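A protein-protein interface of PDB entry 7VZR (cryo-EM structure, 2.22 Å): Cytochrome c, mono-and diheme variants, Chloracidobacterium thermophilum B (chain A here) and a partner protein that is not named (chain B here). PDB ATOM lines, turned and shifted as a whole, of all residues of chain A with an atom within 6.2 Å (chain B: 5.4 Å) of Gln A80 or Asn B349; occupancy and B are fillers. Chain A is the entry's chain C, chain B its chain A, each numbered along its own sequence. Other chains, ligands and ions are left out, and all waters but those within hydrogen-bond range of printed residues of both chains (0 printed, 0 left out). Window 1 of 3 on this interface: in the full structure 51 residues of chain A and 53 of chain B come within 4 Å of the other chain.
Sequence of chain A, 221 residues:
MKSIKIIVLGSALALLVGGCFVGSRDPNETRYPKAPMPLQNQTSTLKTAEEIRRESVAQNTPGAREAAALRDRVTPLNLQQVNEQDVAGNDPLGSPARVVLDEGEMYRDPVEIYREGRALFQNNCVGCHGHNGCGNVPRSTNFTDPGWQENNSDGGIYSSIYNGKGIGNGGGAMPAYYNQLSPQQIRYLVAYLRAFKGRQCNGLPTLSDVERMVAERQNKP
The side-chain amide nitrogen of Asn B336 lies close to the side-chain amide nitrogen of Gln A80, 3.4 Å away.
The guanidinium group (NH1) of Arg B865 is in hydrogen-bond range of the side-chain sulfur (SD) of Met A37.
N of Arg B865 is in hydrogen-bond range of O of Val A82.
OD1 of Asn B349 lies within hydrogen-bond range of ND2 of Asn B336 (3.1 Å).
The side-chain amide oxygen (OD1) of Asn B336 sits at hydrogen-bond distance from the backbone NH (N) of Gly B351, 2.8 Å away.
The backbone NH (N) of Arg B352 is in hydrogen-bond range of the side-chain amide oxygen (OD1) of Asn B349.
The backbone carbonyl oxygen (O) of Arg B865 is in hydrogen-bond range of the backbone NH (N) of Leu B640.
The side-chain amide oxygen (OE1) of Gln A185 sits close to the backbone carbonyl oxygen (O) of Gln A80, at 3.3 Å.
Lys A34 touches Asn B336.
Leu A79 touches Ile B347 (CD2 to O, 3.7 Å).
ND2 of Asn B349 touches NE2 of Gln A80, 3.7 Å away.
Arg B865 touches Gln A80.
Gln A81 touches Gln B863.
Arg B865 touches Gln A81.
Of the printed residues of chain B, Leu A79 touches Ile B347 (3.7 Å).
Printed residues of chain B within 4 Å of Met A37: Arg B865.
Printed residues of chain A within 4 Å of Asn B336: Lys A34 (3.9 Å) and Gln A80 (3.4 Å).
Of the printed residues of chain B, Lys A34 touches Asn B336 (3.9 Å).
Printed residues of chain B within 4 Å of Val A82: Arg B865 (3.0 Å).
Phe B861 touches none of the printed residues of chain A.
The nearest printed residue of chain B that does not touch Gln A80 is Val B348 (4.5 Å).
Of the 13 printed residues of chain B, 5 touch a printed residue of chain A.
Of the 10 printed residues of chain A, 6 touch a printed residue of chain B.
Printed residues of chain A that touch a printed residue of chain B: Lys A34, Met A37, Leu A79, Gln A80, Gln A81 and Val A82.
Hydrophobic or aromatic side chains of chain A within 4 Å of the printed part of chain B: Met A37 and Leu A79.
Along chain A the printed residues that touch a printed residue of chain B span positions 34 to 82.
Among the printed residues, 9 pairs touch across the chains.
Among the printed residues, no Asp or Glu carboxylate lies within 4 Å of a Lys or Arg side-chain nitrogen of the other chain.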
ATOM      1  N   LYS A  34      28.726  21.734   4.770  1.00  0.00           N
ATOM      2  CA  LYS A  34      27.669  21.724   3.774  1.00  0.00           C
ATOM      3  C   LYS A  34      26.332  21.909   4.463  1.00  0.00           C
ATOM      4  O   LYS A  34      26.231  21.696   5.641  1.00  0.00           O
ATOM      5  CB  LYS A  34      27.726  20.440   2.949  1.00  0.00           C
ATOM      6  CG  LYS A  34      27.484  19.146   3.632  1.00  0.00           C
ATOM      7  CD  LYS A  34      27.012  18.188   2.673  1.00  0.00           C
ATOM      8  CE  LYS A  34      26.828  16.837   3.220  1.00  0.00           C
ATOM      9  NZ  LYS A  34      25.467  16.551   3.376  1.00  0.00           N
ATOM     10  N   MET A  37      21.248  17.550   5.305  1.00  0.00           N
ATOM     11  CA  MET A  37      20.340  16.747   4.458  1.00  0.00           C
ATOM     12  C   MET A  37      18.899  17.095   4.859  1.00  0.00           C
ATOM     13  O   MET A  37      18.601  17.082   6.061  1.00  0.00           O
ATOM     14  CB  MET A  37      20.564  15.242   4.613  1.00  0.00           C
ATOM     15  CG  MET A  37      19.679  14.428   3.690  1.00  0.00           C
ATOM     16  SD  MET A  37      20.089  12.669   3.705  1.00  0.00           S
ATOM     17  CE  MET A  37      21.806  12.775   3.221  1.00  0.00           C
ATOM     18  N   LEU A  77      27.379  15.863  -1.389  1.00  0.00           N
ATOM     19  CA  LEU A  77      26.009  16.123  -0.895  1.00  0.00           C
ATOM     20  C   LEU A  77      25.019  14.941  -0.820  1.00  0.00           C
ATOM     21  O   LEU A  77      24.013  15.046  -0.164  1.00  0.00           O
ATOM     22  CB  LEU A  77      25.354  17.188  -1.752  1.00  0.00           C
ATOM     23  CG  LEU A  77      25.558  18.700  -1.652  1.00  0.00           C
ATOM     24  CD1 LEU A  77      26.818  19.113  -1.153  1.00  0.00           C
ATOM     25  CD2 LEU A  77      25.353  19.268  -3.015  1.00  0.00           C
ATOM     26  N   ASN A  78      25.180  13.905  -1.601  1.00  0.00           N
ATOM     27  CA  ASN A  78      24.315  12.724  -1.675  1.00  0.00           C
ATOM     28  C   ASN A  78      25.056  11.417  -1.487  1.00  0.00           C
ATOM     29  O   ASN A  78      24.876  10.508  -2.250  1.00  0.00           O
ATOM     30  CB  ASN A  78      23.591  12.660  -3.003  1.00  0.00           C
ATOM     31  CG  ASN A  78      23.148  13.931  -3.443  1.00  0.00           C
ATOM     32  OD1 ASN A  78      23.680  14.511  -4.357  1.00  0.00           O
ATOM     33  ND2 ASN A  78      22.161  14.428  -2.795  1.00  0.00           N
ATOM     34  N   LEU A  79      25.883  11.308  -0.472  1.00  0.00           N
ATOM     35  CA  LEU A  79      26.677  10.155  -0.105  1.00  0.00           C
ATOM     36  C   LEU A  79      26.007   9.340   0.945  1.00  0.00           C
ATOM     37  O   LEU A  79      26.236   8.157   1.009  1.00  0.00           O
ATOM     38  CB  LEU A  79      28.048  10.562   0.451  1.00  0.00           C
ATOM     39  CG  LEU A  79      29.068   9.519   0.901  1.00  0.00           C
ATOM     40  CD1 LEU A  79      29.254   8.597  -0.209  1.00  0.00           C
ATOM     41  CD2 LEU A  79      30.339  10.054   1.555  1.00  0.00           C
ATOM     42  N   GLN A  80      25.289  10.024   1.792  1.00  0.00           N
ATOM     43  CA  GLN A  80      24.622   9.351   2.914  1.00  0.00           C
ATOM     44  C   GLN A  80      23.472   8.498   2.434  1.00  0.00           C
ATOM     45  O   GLN A  80      22.797   8.898   1.473  1.00  0.00           O
ATOM     46  CB  GLN A  80      24.093  10.420   3.874  1.00  0.00           C
ATOM     47  CG  GLN A  80      24.583  10.279   5.308  1.00  0.00           C
ATOM     48  CD  GLN A  80      23.955  11.295   6.236  1.00  0.00           C
ATOM     49  OE1 GLN A  80      24.211  12.492   6.149  1.00  0.00           O
ATOM     50  NE2 GLN A  80      23.122  10.820   7.146  1.00  0.00           N
ATOM     51  N   GLN A  81      23.330   7.328   3.017  1.00  0.00           N
ATOM     52  CA  GLN A  81      22.106   6.584   2.801  1.00  0.00           C
ATOM     53  C   GLN A  81      20.950   7.542   2.959  1.00  0.00           C
ATOM     54  O   GLN A  81      21.024   8.516   3.670  1.00  0.00           O
ATOM     55  CB  GLN A  81      21.964   5.394   3.741  1.00  0.00           C
ATOM     56  CG  GLN A  81      22.989   4.388   3.737  1.00  0.00           C
ATOM     57  CD  GLN A  81      23.249   3.779   2.425  1.00  0.00           C
ATOM     58  OE1 GLN A  81      22.440   3.104   1.814  1.00  0.00           O
ATOM     59  NE2 GLN A  81      24.389   4.016   1.978  1.00  0.00           N
ATOM     60  N   VAL A  82      19.881   7.273   2.276  1.00  0.00           N
ATOM     61  CA  VAL A  82      18.874   8.239   1.917  1.00  0.00           C
ATOM     62  C   VAL A  82      17.651   7.833   2.696  1.00  0.00           C
ATOM     63  O   VAL A  82      17.647   6.730   3.209  1.00  0.00           O
ATOM     64  CB  VAL A  82      18.734   8.235   0.393  1.00  0.00           C
ATOM     65  CG1 VAL A  82      17.516   7.629  -0.180  1.00  0.00           C
ATOM     66  CG2 VAL A  82      19.179   9.462  -0.163  1.00  0.00           C
ATOM     67  N   LEU A 120      30.458   7.699  -4.063  1.00  0.00           N
ATOM     68  CA  LEU A 120      29.587   6.541  -4.010  1.00  0.00           C
ATOM     69  C   LEU A 120      30.286   5.294  -4.486  1.00  0.00           C
ATOM     70  O   LEU A 120      30.206   4.276  -3.836  1.00  0.00           O
ATOM     71  CB  LEU A 120      28.326   6.767  -4.803  1.00  0.00           C
ATOM     72  CG  LEU A 120      27.228   7.516  -4.068  1.00  0.00           C
ATOM     73  CD1 LEU A 120      26.385   8.024  -5.092  1.00  0.00           C
ATOM     74  CD2 LEU A 120      26.502   6.723  -3.045  1.00  0.00           C
ATOM     75  N   GLN A 185      20.965   8.891  -6.761  1.00  0.00           N
ATOM     76  CA  GLN A 185      22.208   8.298  -6.492  1.00  0.00           C
ATOM     77  C   GLN A 185      22.583   7.322  -7.642  1.00  0.00           C
ATOM     78  O   GLN A 185      23.636   7.358  -8.028  1.00  0.00           O
ATOM     79  CB  GLN A 185      22.214   7.659  -5.120  1.00  0.00           C
ATOM     80  CG  GLN A 185      22.436   8.581  -3.982  1.00  0.00           C
ATOM     81  CD  GLN A 185      22.298   7.962  -2.679  1.00  0.00           C
ATOM     82  OE1 GLN A 185      22.967   8.214  -1.735  1.00  0.00           O
ATOM     83  NE2 GLN A 185      21.480   7.182  -2.637  1.00  0.00           N
ATOM     84  N   ASN B 336      28.222  14.481  10.106  1.00  0.00           N
ATOM     85  CA  ASN B 336      27.846  14.178   8.713  1.00  0.00           C
ATOM     86  C   ASN B 336      27.902  15.382   7.791  1.00  0.00           C
ATOM     87  O   ASN B 336      27.939  15.234   6.583  1.00  0.00           O
ATOM     88  CB  ASN B 336      26.469  13.558   8.591  1.00  0.00           C
ATOM     89  CG  ASN B 336      26.314  12.350   9.406  1.00  0.00           C
ATOM     90  OD1 ASN B 336      27.237  11.863   9.902  1.00  0.00           O
ATOM     91  ND2 ASN B 336      25.139  11.961   9.639  1.00  0.00           N
ATOM     92  N   ILE B 347      33.466   8.939   4.847  1.00  0.00           N
ATOM     93  CA  ILE B 347      32.702   7.979   5.595  1.00  0.00           C
ATOM     94  C   ILE B 347      31.235   8.242   5.361  1.00  0.00           C
ATOM     95  O   ILE B 347      30.832   9.376   5.186  1.00  0.00           O
ATOM     96  CB  ILE B 347      33.090   8.028   7.081  1.00  0.00           C
ATOM     97  CG1 ILE B 347      34.619   8.089   7.148  1.00  0.00           C
ATOM     98  CG2 ILE B 347      32.451   6.882   7.863  1.00  0.00           C
ATOM     99  CD1 ILE B 347      35.392   6.869   6.749  1.00  0.00           C
ATOM    100  N   VAL B 348      30.463   7.179   5.280  1.00  0.00           N
ATOM    101  CA  VAL B 348      29.018   7.219   5.213  1.00  0.00           C
ATOM    102  C   VAL B 348      28.485   7.333   6.622  1.00  0.00           C
ATOM    103  O   VAL B 348      28.855   6.542   7.467  1.00  0.00           O
ATOM    104  CB  VAL B 348      28.482   5.976   4.487  1.00  0.00           C
ATOM    105  CG1 VAL B 348      26.972   5.858   4.585  1.00  0.00           C
ATOM    106  CG2 VAL B 348      28.883   6.015   3.162  1.00  0.00           C
ATOM    107  N   ASN B 349      27.800   8.406   6.905  1.00  0.00           N
ATOM    108  CA  ASN B 349      27.255   8.680   8.223  1.00  0.00           C
ATOM    109  C   ASN B 349      28.304   8.537   9.345  1.00  0.00           C
ATOM    110  O   ASN B 349      28.205   7.662  10.200  1.00  0.00           O
ATOM    111  CB  ASN B 349      26.040   7.801   8.474  1.00  0.00           C
ATOM    112  CG  ASN B 349      25.144   8.345   9.512  1.00  0.00           C
ATOM    113  OD1 ASN B 349      25.585   9.003  10.415  1.00  0.00           O
ATOM    114  ND2 ASN B 349      23.898   8.032   9.426  1.00  0.00           N
ATOM    115  N   PRO B 350      29.300   9.407   9.387  1.00  0.00           N
ATOM    116  CA  PRO B 350      30.222   9.402  10.516  1.00  0.00           C
ATOM    117  C   PRO B 350      29.576   9.679  11.870  1.00  0.00           C
ATOM    118  O   PRO B 350      30.068   9.181  12.851  1.00  0.00           O
ATOM    119  CB  PRO B 350      31.203  10.497  10.122  1.00  0.00           C
ATOM    120  CG  PRO B 350      30.580  11.188   9.199  1.00  0.00           C
ATOM    121  CD  PRO B 350      29.740  10.385   8.406  1.00  0.00           C
ATOM    122  N   GLY B 351      28.518  10.439  11.930  1.00  0.00           N
ATOM    123  CA  GLY B 351      27.821  10.746  13.147  1.00  0.00           C
ATOM    124  C   GLY B 351      27.442   9.567  13.975  1.00  0.00           C
ATOM    125  O   GLY B 351      27.880   9.428  15.110  1.00  0.00           O
ATOM    126  N   ARG B 352      26.661   8.697  13.357  1.00  0.00           N
ATOM    127  CA  ARG B 352      26.255   7.435  13.916  1.00  0.00           C
ATOM    128  C   ARG B 352      27.416   6.474  14.100  1.00  0.00           C
ATOM    129  O   ARG B 352      27.399   5.710  15.033  1.00  0.00           O
ATOM    130  CB  ARG B 352      25.192   6.811  13.017  1.00  0.00           C
ATOM    131  CG  ARG B 352      23.874   6.329  13.593  1.00  0.00           C
ATOM    132  CD  ARG B 352      23.561   6.535  15.101  1.00  0.00           C
ATOM    133  NE  ARG B 352      22.218   7.014  15.335  1.00  0.00           N
ATOM    134  CZ  ARG B 352      21.115   6.276  15.308  1.00  0.00           C
ATOM    135  NH1 ARG B 352      21.162   5.049  14.997  1.00  0.00           N
ATOM    136  NH2 ARG B 352      19.959   6.810  15.455  1.00  0.00           N
ATOM    137  N   MET B 353      28.448   6.532  13.292  1.00  0.00           N
ATOM    138  CA  MET B 353      29.598   5.661  13.539  1.00  0.00           C
ATOM    139  C   MET B 353      30.310   6.008  14.859  1.00  0.00           C
ATOM    140  O   MET B 353      30.649   5.126  15.616  1.00  0.00           O
ATOM    141  CB  MET B 353      30.562   5.685  12.352  1.00  0.00           C
ATOM    142  CG  MET B 353      31.835   4.903  12.495  1.00  0.00           C
ATOM    143  SD  MET B 353      32.953   5.083  11.146  1.00  0.00           S
ATOM    144  CE  MET B 353      33.754   6.608  11.520  1.00  0.00           C
ATOM    145  N   LEU B 640      16.318   7.149  11.584  1.00  0.00           N
ATOM    146  CA  LEU B 640      17.579   7.901  11.563  1.00  0.00           C
ATOM    147  C   LEU B 640      17.390   9.311  11.635  1.00  0.00           C
ATOM    148  O   LEU B 640      18.189   9.927  12.019  1.00  0.00           O
ATOM    149  CB  LEU B 640      18.497   7.600  10.459  1.00  0.00           C
ATOM    150  CG  LEU B 640      19.738   6.900  10.861  1.00  0.00           C
ATOM    151  CD1 LEU B 640      19.381   5.925  11.898  1.00  0.00           C
ATOM    152  CD2 LEU B 640      20.231   6.264   9.631  1.00  0.00           C
ATOM    153  N   GLY B 860      31.693   2.534   8.648  1.00  0.00           N
ATOM    154  CA  GLY B 860      30.658   3.507   8.451  1.00  0.00           C
ATOM    155  C   GLY B 860      29.313   2.905   8.836  1.00  0.00           C
ATOM    156  O   GLY B 860      29.242   1.830   9.063  1.00  0.00           O
ATOM    157  N   PHE B 861      28.246   3.565   8.851  1.00  0.00           N
ATOM    158  CA  PHE B 861      26.959   3.096   9.225  1.00  0.00           C
ATOM    159  C   PHE B 861      26.059   3.211   8.022  1.00  0.00           C
ATOM    160  O   PHE B 861      25.964   4.197   7.542  1.00  0.00           O
ATOM    161  CB  PHE B 861      26.530   3.819  10.523  1.00  0.00           C
ATOM    162  CG  PHE B 861      25.202   3.479  10.994  1.00  0.00           C
ATOM    163  CD1 PHE B 861      24.962   2.370  11.723  1.00  0.00           C
ATOM    164  CD2 PHE B 861      24.165   4.339  10.767  1.00  0.00           C
ATOM    165  CE1 PHE B 861      23.728   2.085  12.166  1.00  0.00           C
ATOM    166  CE2 PHE B 861      22.901   4.039  11.226  1.00  0.00           C
ATOM    167  CZ  PHE B 861      22.713   2.954  11.938  1.00  0.00           C
ATOM    168  N   GLN B 863      22.637   2.027   7.476  1.00  0.00           N
ATOM    169  CA  GLN B 863      21.195   1.938   7.466  1.00  0.00           C
ATOM    170  C   GLN B 863      20.588   3.199   6.833  1.00  0.00           C
ATOM    171  O   GLN B 863      21.076   4.301   7.015  1.00  0.00           O
ATOM    172  CB  GLN B 863      20.706   1.651   8.876  1.00  0.00           C
ATOM    173  CG  GLN B 863      19.245   1.406   9.030  1.00  0.00           C
ATOM    174  CD  GLN B 863      18.913   0.935  10.383  1.00  0.00           C
ATOM    175  OE1 GLN B 863      18.732   1.706  11.257  1.00  0.00           O
ATOM    176  NE2 GLN B 863      18.856  -0.349  10.568  1.00  0.00           N
ATOM    177  N   ARG B 865      18.056   6.217   6.116  1.00  0.00           N
ATOM    178  CA  ARG B 865      17.866   7.265   7.060  1.00  0.00           C
ATOM    179  C   ARG B 865      16.418   7.554   7.326  1.00  0.00           C
ATOM    180  O   ARG B 865      15.929   7.380   8.453  1.00  0.00           O
ATOM    181  CB  ARG B 865      18.576   8.496   6.579  1.00  0.00           C
ATOM    182  CG  ARG B 865      18.390   9.650   7.367  1.00  0.00           C
ATOM    183  CD  ARG B 865      19.147  10.773   6.852  1.00  0.00           C
ATOM    184  NE  ARG B 865      18.601  12.051   7.277  1.00  0.00           N
ATOM    185  CZ  ARG B 865      17.614  12.633   6.640  1.00  0.00           C
ATOM    186  NH1 ARG B 865      17.148  12.115   5.577  1.00  0.00           N
ATOM    187  NH2 ARG B 865      17.140  13.761   6.982  1.00  0.00           N
